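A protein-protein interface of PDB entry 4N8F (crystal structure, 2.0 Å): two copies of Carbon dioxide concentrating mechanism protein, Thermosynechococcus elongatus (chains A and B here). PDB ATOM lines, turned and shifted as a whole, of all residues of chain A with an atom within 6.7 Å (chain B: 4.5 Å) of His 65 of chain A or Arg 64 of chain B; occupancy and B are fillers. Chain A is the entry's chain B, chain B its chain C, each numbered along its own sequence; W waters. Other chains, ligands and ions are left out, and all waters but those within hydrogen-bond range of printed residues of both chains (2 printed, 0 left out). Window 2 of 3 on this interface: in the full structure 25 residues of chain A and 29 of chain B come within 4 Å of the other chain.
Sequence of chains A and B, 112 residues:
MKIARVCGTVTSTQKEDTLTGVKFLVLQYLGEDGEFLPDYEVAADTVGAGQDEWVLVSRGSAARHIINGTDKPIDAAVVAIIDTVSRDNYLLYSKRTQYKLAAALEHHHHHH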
ATOM      1  N   GLY A  60      12.841  34.332  -0.075  1.00  0.00           N
ATOM      2  CA  GLY A  60      14.064  33.781  -0.694  1.00  0.00           C
ATOM      3  C   GLY A  60      13.927  32.296  -1.004  1.00  0.00           C
ATOM      4  O   GLY A  60      12.809  31.744  -1.123  1.00  0.00           O
ATOM      5  N   SER A  61      15.071  31.618  -1.037  1.00  0.00           N
ATOM      6  CA  SER A  61      15.130  30.228  -1.452  1.00  0.00           C
ATOM      7  C   SER A  61      14.393  29.279  -0.490  1.00  0.00           C
ATOM      8  O   SER A  61      14.128  28.126  -0.822  1.00  0.00           O
ATOM      9  CB  SER A  61      16.583  29.782  -1.629  1.00  0.00           C
ATOM     10  OG  SER A  61      17.330  30.042  -0.491  1.00  0.00           O
ATOM     11  N   ALA A  62      14.101  29.760   0.690  1.00  0.00           N
ATOM     12  CA  ALA A  62      13.314  29.012   1.613  1.00  0.00           C
ATOM     13  C   ALA A  62      11.999  28.610   1.019  1.00  0.00           C
ATOM     14  O   ALA A  62      11.468  27.578   1.388  1.00  0.00           O
ATOM     15  CB  ALA A  62      13.038  29.839   2.862  1.00  0.00           C
ATOM     16  N   ALA A  63      11.454  29.448   0.154  1.00  0.00           N
ATOM     17  CA  ALA A  63      10.205  29.190  -0.479  1.00  0.00           C
ATOM     18  C   ALA A  63      10.249  27.933  -1.373  1.00  0.00           C
ATOM     19  O   ALA A  63       9.248  27.236  -1.517  1.00  0.00           O
ATOM     20  CB  ALA A  63       9.754  30.385  -1.292  1.00  0.00           C
ATOM     21  N   ARG A  64      11.412  27.632  -1.930  1.00  0.00           N
ATOM     22  CA  ARG A  64      11.535  26.448  -2.746  1.00  0.00           C
ATOM     23  C   ARG A  64      11.530  25.192  -1.904  1.00  0.00           C
ATOM     24  O   ARG A  64      11.564  24.094  -2.478  1.00  0.00           O
ATOM     25  CB  ARG A  64      12.770  26.487  -3.643  1.00  0.00           C
ATOM     26  CG  ARG A  64      12.714  27.715  -4.569  1.00  0.00           C
ATOM     27  CD  ARG A  64      13.617  27.578  -5.747  1.00  0.00           C
ATOM     28  NE  ARG A  64      15.015  27.299  -5.443  1.00  0.00           N
ATOM     29  CZ  ARG A  64      16.008  28.150  -5.146  1.00  0.00           C
ATOM     30  NH1 ARG A  64      15.840  29.439  -5.018  1.00  0.00           N
ATOM     31  NH2 ARG A  64      17.219  27.651  -4.987  1.00  0.00           N
ATOM     32  N   HIS A  65      11.497  25.334  -0.578  1.00  0.00           N
ATOM     33  CA  HIS A  65      11.547  24.154   0.288  1.00  0.00           C
ATOM     34  C   HIS A  65      10.187  23.766   0.932  1.00  0.00           C
ATOM     35  O   HIS A  65      10.120  22.819   1.773  1.00  0.00           O
ATOM     36  CB  HIS A  65      12.657  24.238   1.328  1.00  0.00           C
ATOM     37  CG  HIS A  65      14.018  24.103   0.728  1.00  0.00           C
ATOM     38  ND1 HIS A  65      14.633  25.150   0.059  1.00  0.00           N
ATOM     39  CD2 HIS A  65      14.879  23.061   0.677  1.00  0.00           C
ATOM     40  CE1 HIS A  65      15.806  24.748  -0.409  1.00  0.00           C
ATOM     41  NE2 HIS A  65      15.979  23.481  -0.046  1.00  0.00           N
ATOM     42  N   ILE A  66       9.147  24.400   0.469  1.00  0.00           N
ATOM     43  CA  ILE A  66       7.774  23.880   0.681  1.00  0.00           C
ATOM     44  C   ILE A  66       7.571  22.589  -0.085  1.00  0.00           C
ATOM     45  O   ILE A  66       8.373  22.212  -0.953  1.00  0.00           O
ATOM     46  CB  ILE A  66       6.675  24.934   0.302  1.00  0.00           C
ATOM     47  CG1 ILE A  66       6.609  25.178  -1.224  1.00  0.00           C
ATOM     48  CG2 ILE A  66       6.902  26.249   1.086  1.00  0.00           C
ATOM     49  CD1 ILE A  66       5.756  26.352  -1.621  1.00  0.00           C
ATOM     50  N   ILE A  67       6.497  21.886   0.263  1.00  0.00           N
ATOM     51  CA  ILE A  67       6.182  20.630  -0.367  1.00  0.00           C
ATOM     52  C   ILE A  67       6.053  20.886  -1.849  1.00  0.00           C
ATOM     53  O   ILE A  67       5.475  21.881  -2.263  1.00  0.00           O
ATOM     54  CB  ILE A  67       4.932  19.956   0.281  1.00  0.00           C
ATOM     55  CG1 ILE A  67       4.671  18.604  -0.335  1.00  0.00           C
ATOM     56  CG2 ILE A  67       3.678  20.845   0.176  1.00  0.00           C
ATOM     57  CD1 ILE A  67       3.487  17.882   0.335  1.00  0.00           C
ATOM     58  N   ASN A  68       6.624  19.981  -2.631  1.00  0.00           N
ATOM     59  CA  ASN A  68       6.767  20.100  -4.096  1.00  0.00           C
ATOM     60  C   ASN A  68       7.385  21.407  -4.679  1.00  0.00           C
ATOM     61  O   ASN A  68       7.193  21.735  -5.844  1.00  0.00           O
ATOM     62  CB  ASN A  68       5.454  19.728  -4.809  1.00  0.00           C
ATOM     63  CG  ASN A  68       5.700  19.120  -6.223  1.00  0.00           C
ATOM     64  OD1 ASN A  68       6.523  18.192  -6.417  1.00  0.00           O
ATOM     65  ND2 ASN A  68       4.980  19.660  -7.228  1.00  0.00           N
ATOM     66  N   GLY A  69       8.146  22.132  -3.871  1.00  0.00           N
ATOM     67  CA  GLY A  69       8.569  23.475  -4.219  1.00  0.00           C
ATOM     68  C   GLY A  69       9.854  23.474  -5.003  1.00  0.00           C
ATOM     69  O   GLY A  69      10.265  24.521  -5.493  1.00  0.00           O
ATOM     70  N   THR A  70      10.490  22.306  -5.125  1.00  0.00           N
ATOM     71  CA  THR A  70      11.802  22.210  -5.736  1.00  0.00           C
ATOM     72  C   THR A  70      11.817  22.799  -7.114  1.00  0.00           C
ATOM     73  O   THR A  70      10.967  22.489  -7.926  1.00  0.00           O
ATOM     74  CB  THR A  70      12.176  20.762  -5.898  1.00  0.00           C
ATOM     75  OG1 THR A  70      12.233  20.173  -4.599  1.00  0.00           O
ATOM     76  CG2 THR A  70      13.538  20.628  -6.595  1.00  0.00           C
ATOM     77  N   ILE A  74       9.801  30.684  -7.180  1.00  0.00           N
ATOM     78  CA  ILE A  74       9.108  31.415  -6.178  1.00  0.00           C
ATOM     79  C   ILE A  74      10.020  31.902  -5.099  1.00  0.00           C
ATOM     80  O   ILE A  74      10.964  31.166  -4.705  1.00  0.00           O
ATOM     81  CB  ILE A  74       7.970  30.564  -5.581  1.00  0.00           C
ATOM     82  CG1 ILE A  74       8.439  29.244  -4.944  1.00  0.00           C
ATOM     83  CG2 ILE A  74       6.936  30.304  -6.654  1.00  0.00           C
ATOM     84  CD1 ILE A  74       7.312  28.429  -4.377  1.00  0.00           C
ATOM     85  N   SER B  61      19.150  31.887   3.354  1.00  0.00           N
ATOM     86  CA  SER B  61      19.432  30.488   3.318  1.00  0.00           C
ATOM     87  C   SER B  61      20.386  30.070   4.439  1.00  0.00           C
ATOM     88  O   SER B  61      20.430  28.861   4.775  1.00  0.00           O
ATOM     89  CB  SER B  61      19.947  30.117   1.952  1.00  0.00           C
ATOM     90  OG  SER B  61      21.160  30.804   1.635  1.00  0.00           O
ATOM     91  N   ALA B  62      21.052  31.035   5.085  1.00  0.00           N
ATOM     92  CA  ALA B  62      21.848  30.740   6.299  1.00  0.00           C
ATOM     93  C   ALA B  62      20.987  29.923   7.301  1.00  0.00           C
ATOM     94  O   ALA B  62      21.486  29.076   7.989  1.00  0.00           O
ATOM     95  CB  ALA B  62      22.315  31.998   6.975  1.00  0.00           C
ATOM     96  N   ALA B  63      19.711  30.254   7.393  1.00  0.00           N
ATOM     97  CA  ALA B  63      18.839  29.604   8.389  1.00  0.00           C
ATOM     98  C   ALA B  63      18.729  28.095   8.222  1.00  0.00           C
ATOM     99  O   ALA B  63      18.387  27.346   9.192  1.00  0.00           O
ATOM    100  CB  ALA B  63      17.466  30.253   8.394  1.00  0.00           C
ATOM    101  N   ARG B  64      18.933  27.620   6.996  1.00  0.00           N
ATOM    102  CA  ARG B  64      18.819  26.207   6.683  1.00  0.00           C
ATOM    103  C   ARG B  64      20.049  25.449   7.054  1.00  0.00           C
ATOM    104  O   ARG B  64      20.037  24.241   7.001  1.00  0.00           O
ATOM    105  CB  ARG B  64      18.457  25.949   5.212  1.00  0.00           C
ATOM    106  CG  ARG B  64      17.107  26.566   4.874  1.00  0.00           C
ATOM    107  CD  ARG B  64      16.522  26.159   3.532  1.00  0.00           C
ATOM    108  NE  ARG B  64      17.466  25.987   2.423  1.00  0.00           N
ATOM    109  CZ  ARG B  64      17.670  26.864   1.443  1.00  0.00           C
ATOM    110  NH1 ARG B  64      17.092  28.081   1.438  1.00  0.00           N
ATOM    111  NH2 ARG B  64      18.506  26.545   0.483  1.00  0.00           N
ATOM    112  N   HIS B  65      21.092  26.169   7.457  1.00  0.00           N
ATOM    113  CA  HIS B  65      22.331  25.545   7.908  1.00  0.00           C
ATOM    114  C   HIS B  65      22.443  25.433   9.424  1.00  0.00           C
ATOM    115  O   HIS B  65      23.472  25.066   9.939  1.00  0.00           O
ATOM    116  CB  HIS B  65      23.459  26.327   7.268  1.00  0.00           C
ATOM    117  CG  HIS B  65      23.566  26.042   5.818  1.00  0.00           C
ATOM    118  ND1 HIS B  65      22.830  26.717   4.866  1.00  0.00           N
ATOM    119  CD2 HIS B  65      24.265  25.113   5.154  1.00  0.00           C
ATOM    120  CE1 HIS B  65      23.092  26.223   3.676  1.00  0.00           C
ATOM    121  NE2 HIS B  65      23.997  25.275   3.826  1.00  0.00           N
ATOM    122  N   ILE B  66      21.390  25.792  10.157  1.00  0.00           N
ATOM    123  CA  ILE B  66      21.328  25.405  11.539  1.00  0.00           C
ATOM    124  C   ILE B  66      21.236  23.867  11.573  1.00  0.00           C
ATOM    125  O   ILE B  66      20.902  23.227  10.594  1.00  0.00           O
ATOM    126  CB  ILE B  66      20.132  26.003  12.318  1.00  0.00           C
ATOM    127  CG1 ILE B  66      18.803  25.481  11.802  1.00  0.00           C
ATOM    128  CG2 ILE B  66      20.191  27.521  12.340  1.00  0.00           C
ATOM    129  CD1 ILE B  66      17.630  26.160  12.477  1.00  0.00           C
ATOM    130  N   GLY B  69      18.583  21.774   9.765  1.00  0.00           N
ATOM    131  CA  GLY B  69      17.783  22.778   9.141  1.00  0.00           C
ATOM    132  C   GLY B  69      17.575  22.573   7.659  1.00  0.00           C
ATOM    133  O   GLY B  69      16.801  23.298   7.038  1.00  0.00           O
ATOM    134  N   THR B  70      18.242  21.565   7.111  1.00  0.00           N
ATOM    135  CA  THR B  70      18.412  21.425   5.676  1.00  0.00           C
ATOM    136  C   THR B  70      17.107  21.507   4.847  1.00  0.00           C
ATOM    137  O   THR B  70      16.994  22.233   3.855  1.00  0.00           O
ATOM    138  CB  THR B  70      19.192  20.135   5.370  1.00  0.00           C
ATOM    139  OG1 THR B  70      20.507  20.230   5.944  1.00  0.00           O
ATOM    140  CG2 THR B  70      19.325  19.955   3.873  1.00  0.00           C
ATOM    141  N   ASP B  71      16.098  20.805   5.241  1.00  0.00           N
ATOM    142  CA  ASP B  71      14.937  20.819   4.345  1.00  0.00           C
ATOM    143  C   ASP B  71      13.877  21.814   4.760  1.00  0.00           C
ATOM    144  O   ASP B  71      12.756  21.773   4.243  1.00  0.00           O
ATOM    145  CB  ASP B  71      14.371  19.394   4.254  1.00  0.00           C
ATOM    146  CG  ASP B  71      15.305  18.458   3.479  1.00  0.00           C
ATOM    147  OD1 ASP B  71      16.020  18.935   2.537  1.00  0.00           O
ATOM    148  OD2 ASP B  71      15.305  17.236   3.818  1.00  0.00           O
ATOM    149  N   LYS B  72      14.190  22.662   5.735  1.00  0.00           N
ATOM    150  CA  LYS B  72      13.157  23.461   6.338  1.00  0.00           C
ATOM    151  C   LYS B  72      12.999  24.782   5.586  1.00  0.00           C
ATOM    152  O   LYS B  72      13.989  25.436   5.265  1.00  0.00           O
ATOM    153  CB  LYS B  72      13.422  23.686   7.823  1.00  0.00           C
ATOM    154  CG  LYS B  72      13.564  22.406   8.667  1.00  0.00           C
ATOM    155  CD  LYS B  72      13.571  22.841  10.120  1.00  0.00           C
ATOM    156  CE  LYS B  72      13.851  21.724  11.138  1.00  0.00           C
ATOM    157  NZ  LYS B  72      13.986  20.356  10.608  1.00  0.00           N
ATOM    158  N   PRO B  73      11.766  25.173   5.281  1.00  0.00           N
ATOM    159  CA  PRO B  73      11.478  26.437   4.585  1.00  0.00           C
ATOM    160  C   PRO B  73      11.503  27.639   5.508  1.00  0.00           C
ATOM    161  O   PRO B  73      10.500  28.334   5.678  1.00  0.00           O
ATOM    162  CB  PRO B  73      10.050  26.228   4.039  1.00  0.00           C
ATOM    163  CG  PRO B  73       9.448  25.196   4.933  1.00  0.00           C
ATOM    164  CD  PRO B  73      10.558  24.354   5.478  1.00  0.00           C
ATOM    165  N   ILE B  74      12.646  27.854   6.135  1.00  0.00           N
ATOM    166  CA  ILE B  74      12.847  28.955   7.092  1.00  0.00           C
ATOM    167  C   ILE B  74      13.897  29.893   6.559  1.00  0.00           C
ATOM    168  O   ILE B  74      14.874  29.447   5.903  1.00  0.00           O
ATOM    169  CB  ILE B  74      13.235  28.463   8.495  1.00  0.00           C
ATOM    170  CG1 ILE B  74      14.403  27.463   8.405  1.00  0.00           C
ATOM    171  CG2 ILE B  74      12.080  27.744   9.155  1.00  0.00           C
ATOM    172  CD1 ILE B  74      15.067  27.267   9.751  1.00  0.00           C
HETATM  173  O   HOH W   1      11.889  20.568   2.048  1.00  0.00           O
HETATM  174  O   HOH W   2      19.614  28.656  -1.523  1.00  0.00           O
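The side-chain hydroxyl (OG) of Ser 61 of chain A sits at hydrogen-bond distance from the guanidinium group (NH1) of Arg 64 of chain B, 2.8 Å away.
O of Ser 61 of chain A is in hydrogen-bond range of ND1 of His 65 of chain A.
A ring nitrogen (ND1) of His 65 of chain B is in hydrogen-bond range of the backbone carbonyl oxygen (O) of Ser 61 of chain B, 3.2 Å away.
The backbone NH of Thr 70 of chain B sits at hydrogen-bond distance from the backbone carbonyl oxygen of Arg 64 of chain B (3.2 Å).
Among the printed residues, merely in contact across the chains: Ser 61 of chain A with Ser 61 of chain B (3.6 Å), Ala 62 of chain A with Arg 64 of chain B (3.5 Å), Ala 62 of chain A with Pro 73 of chain B (3.3 Å), Ala 62 of chain A with Ile 74 of chain B (3.6 Å), His 65 of chain A with Arg 64 of chain B (3.4 Å), His 65 of chain A with Thr 70 of chain B (3.9 Å), His 65 of chain A with Asp 71 of chain B (3.8 Å) and His 65 of chain A with Pro 73 of chain B (3.97 Å).
Printed residues of chain B within 4 Å of Ala 62 of chain A: Arg 64, Pro 73 and Ile 74.
His 65 of chain A touches four residues of chain B.
Of the printed residues of chain A, Ser 61 of chain B touches Ser 61.
Arg 64 of chain B touches just these residues of chain A: Ser 61 (2.8 Å), Ala 62 (3.5 Å) and His 65 (3.4 Å).
Gly 69 of chain B touches none of the printed residues of chain A.
The nearest residue of chain A that does not touch Arg 64 of chain B is Arg 64 of chain A (5.7 Å).
The nearest printed residue of chain B that does not touch Ala 62 of chain A is Lys 72 of chain B (5.1 Å).
Printed residues of chain B that touch a printed residue of chain A: Ser 61, Arg 64, Thr 70, Asp 71, Pro 73 and Ile 74.
Hydrophobic or aromatic side chains of chain B within 4 Å of the printed part of chain A: Pro 73.
Of the 12 printed residues of chain A, 3 touch a printed residue of chain B.
Printed residues of chain A that touch a printed residue of chain B: Ser 61, Ala 62 and His 65.
Along chain A the printed residues that touch a printed residue of chain B span positions 61 to 65.
Among the printed residues, 9 pairs touch across the chains.
Ser 61 of chain A touches its own counterpart, Ser 61 of chain B.
Ser 61 of chain A touches Arg 64 of chain B, but with the chains exchanged Arg 64 of chain A does not touch Ser 61 of chain B (7.9 Å).
Ala 62 of chain A touches Ile 74 of chain B, but with the chains exchanged Ile 74 of chain A does not touch Ala 62 of chain B (14.1 Å).
His 65 of chain A touches Arg 64 of chain B, but with the chains exchanged Arg 64 of chain A does not touch His 65 of chain B (10.6 Å).
Positions printed for both chains: 61, 62, 63, 64, 65, 66, 69, 70 and 74.
Of the 9 pairs that touch across the chains among the printed residues, 1 has its exchanged pair printed and touching as well.
Water W1 lies within hydrogen-bond range of the backbone carbonyl oxygen of Asp 71 of chain B (2.6 Å) and the backbone carbonyl oxygen of His 65 of chain A (2.9 Å).
Water W2 bridges the side-chain hydroxyl of Ser 61 of chain A (2.9 Å) and the guanidinium group of Arg 64 of chain B (3.1 Å).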
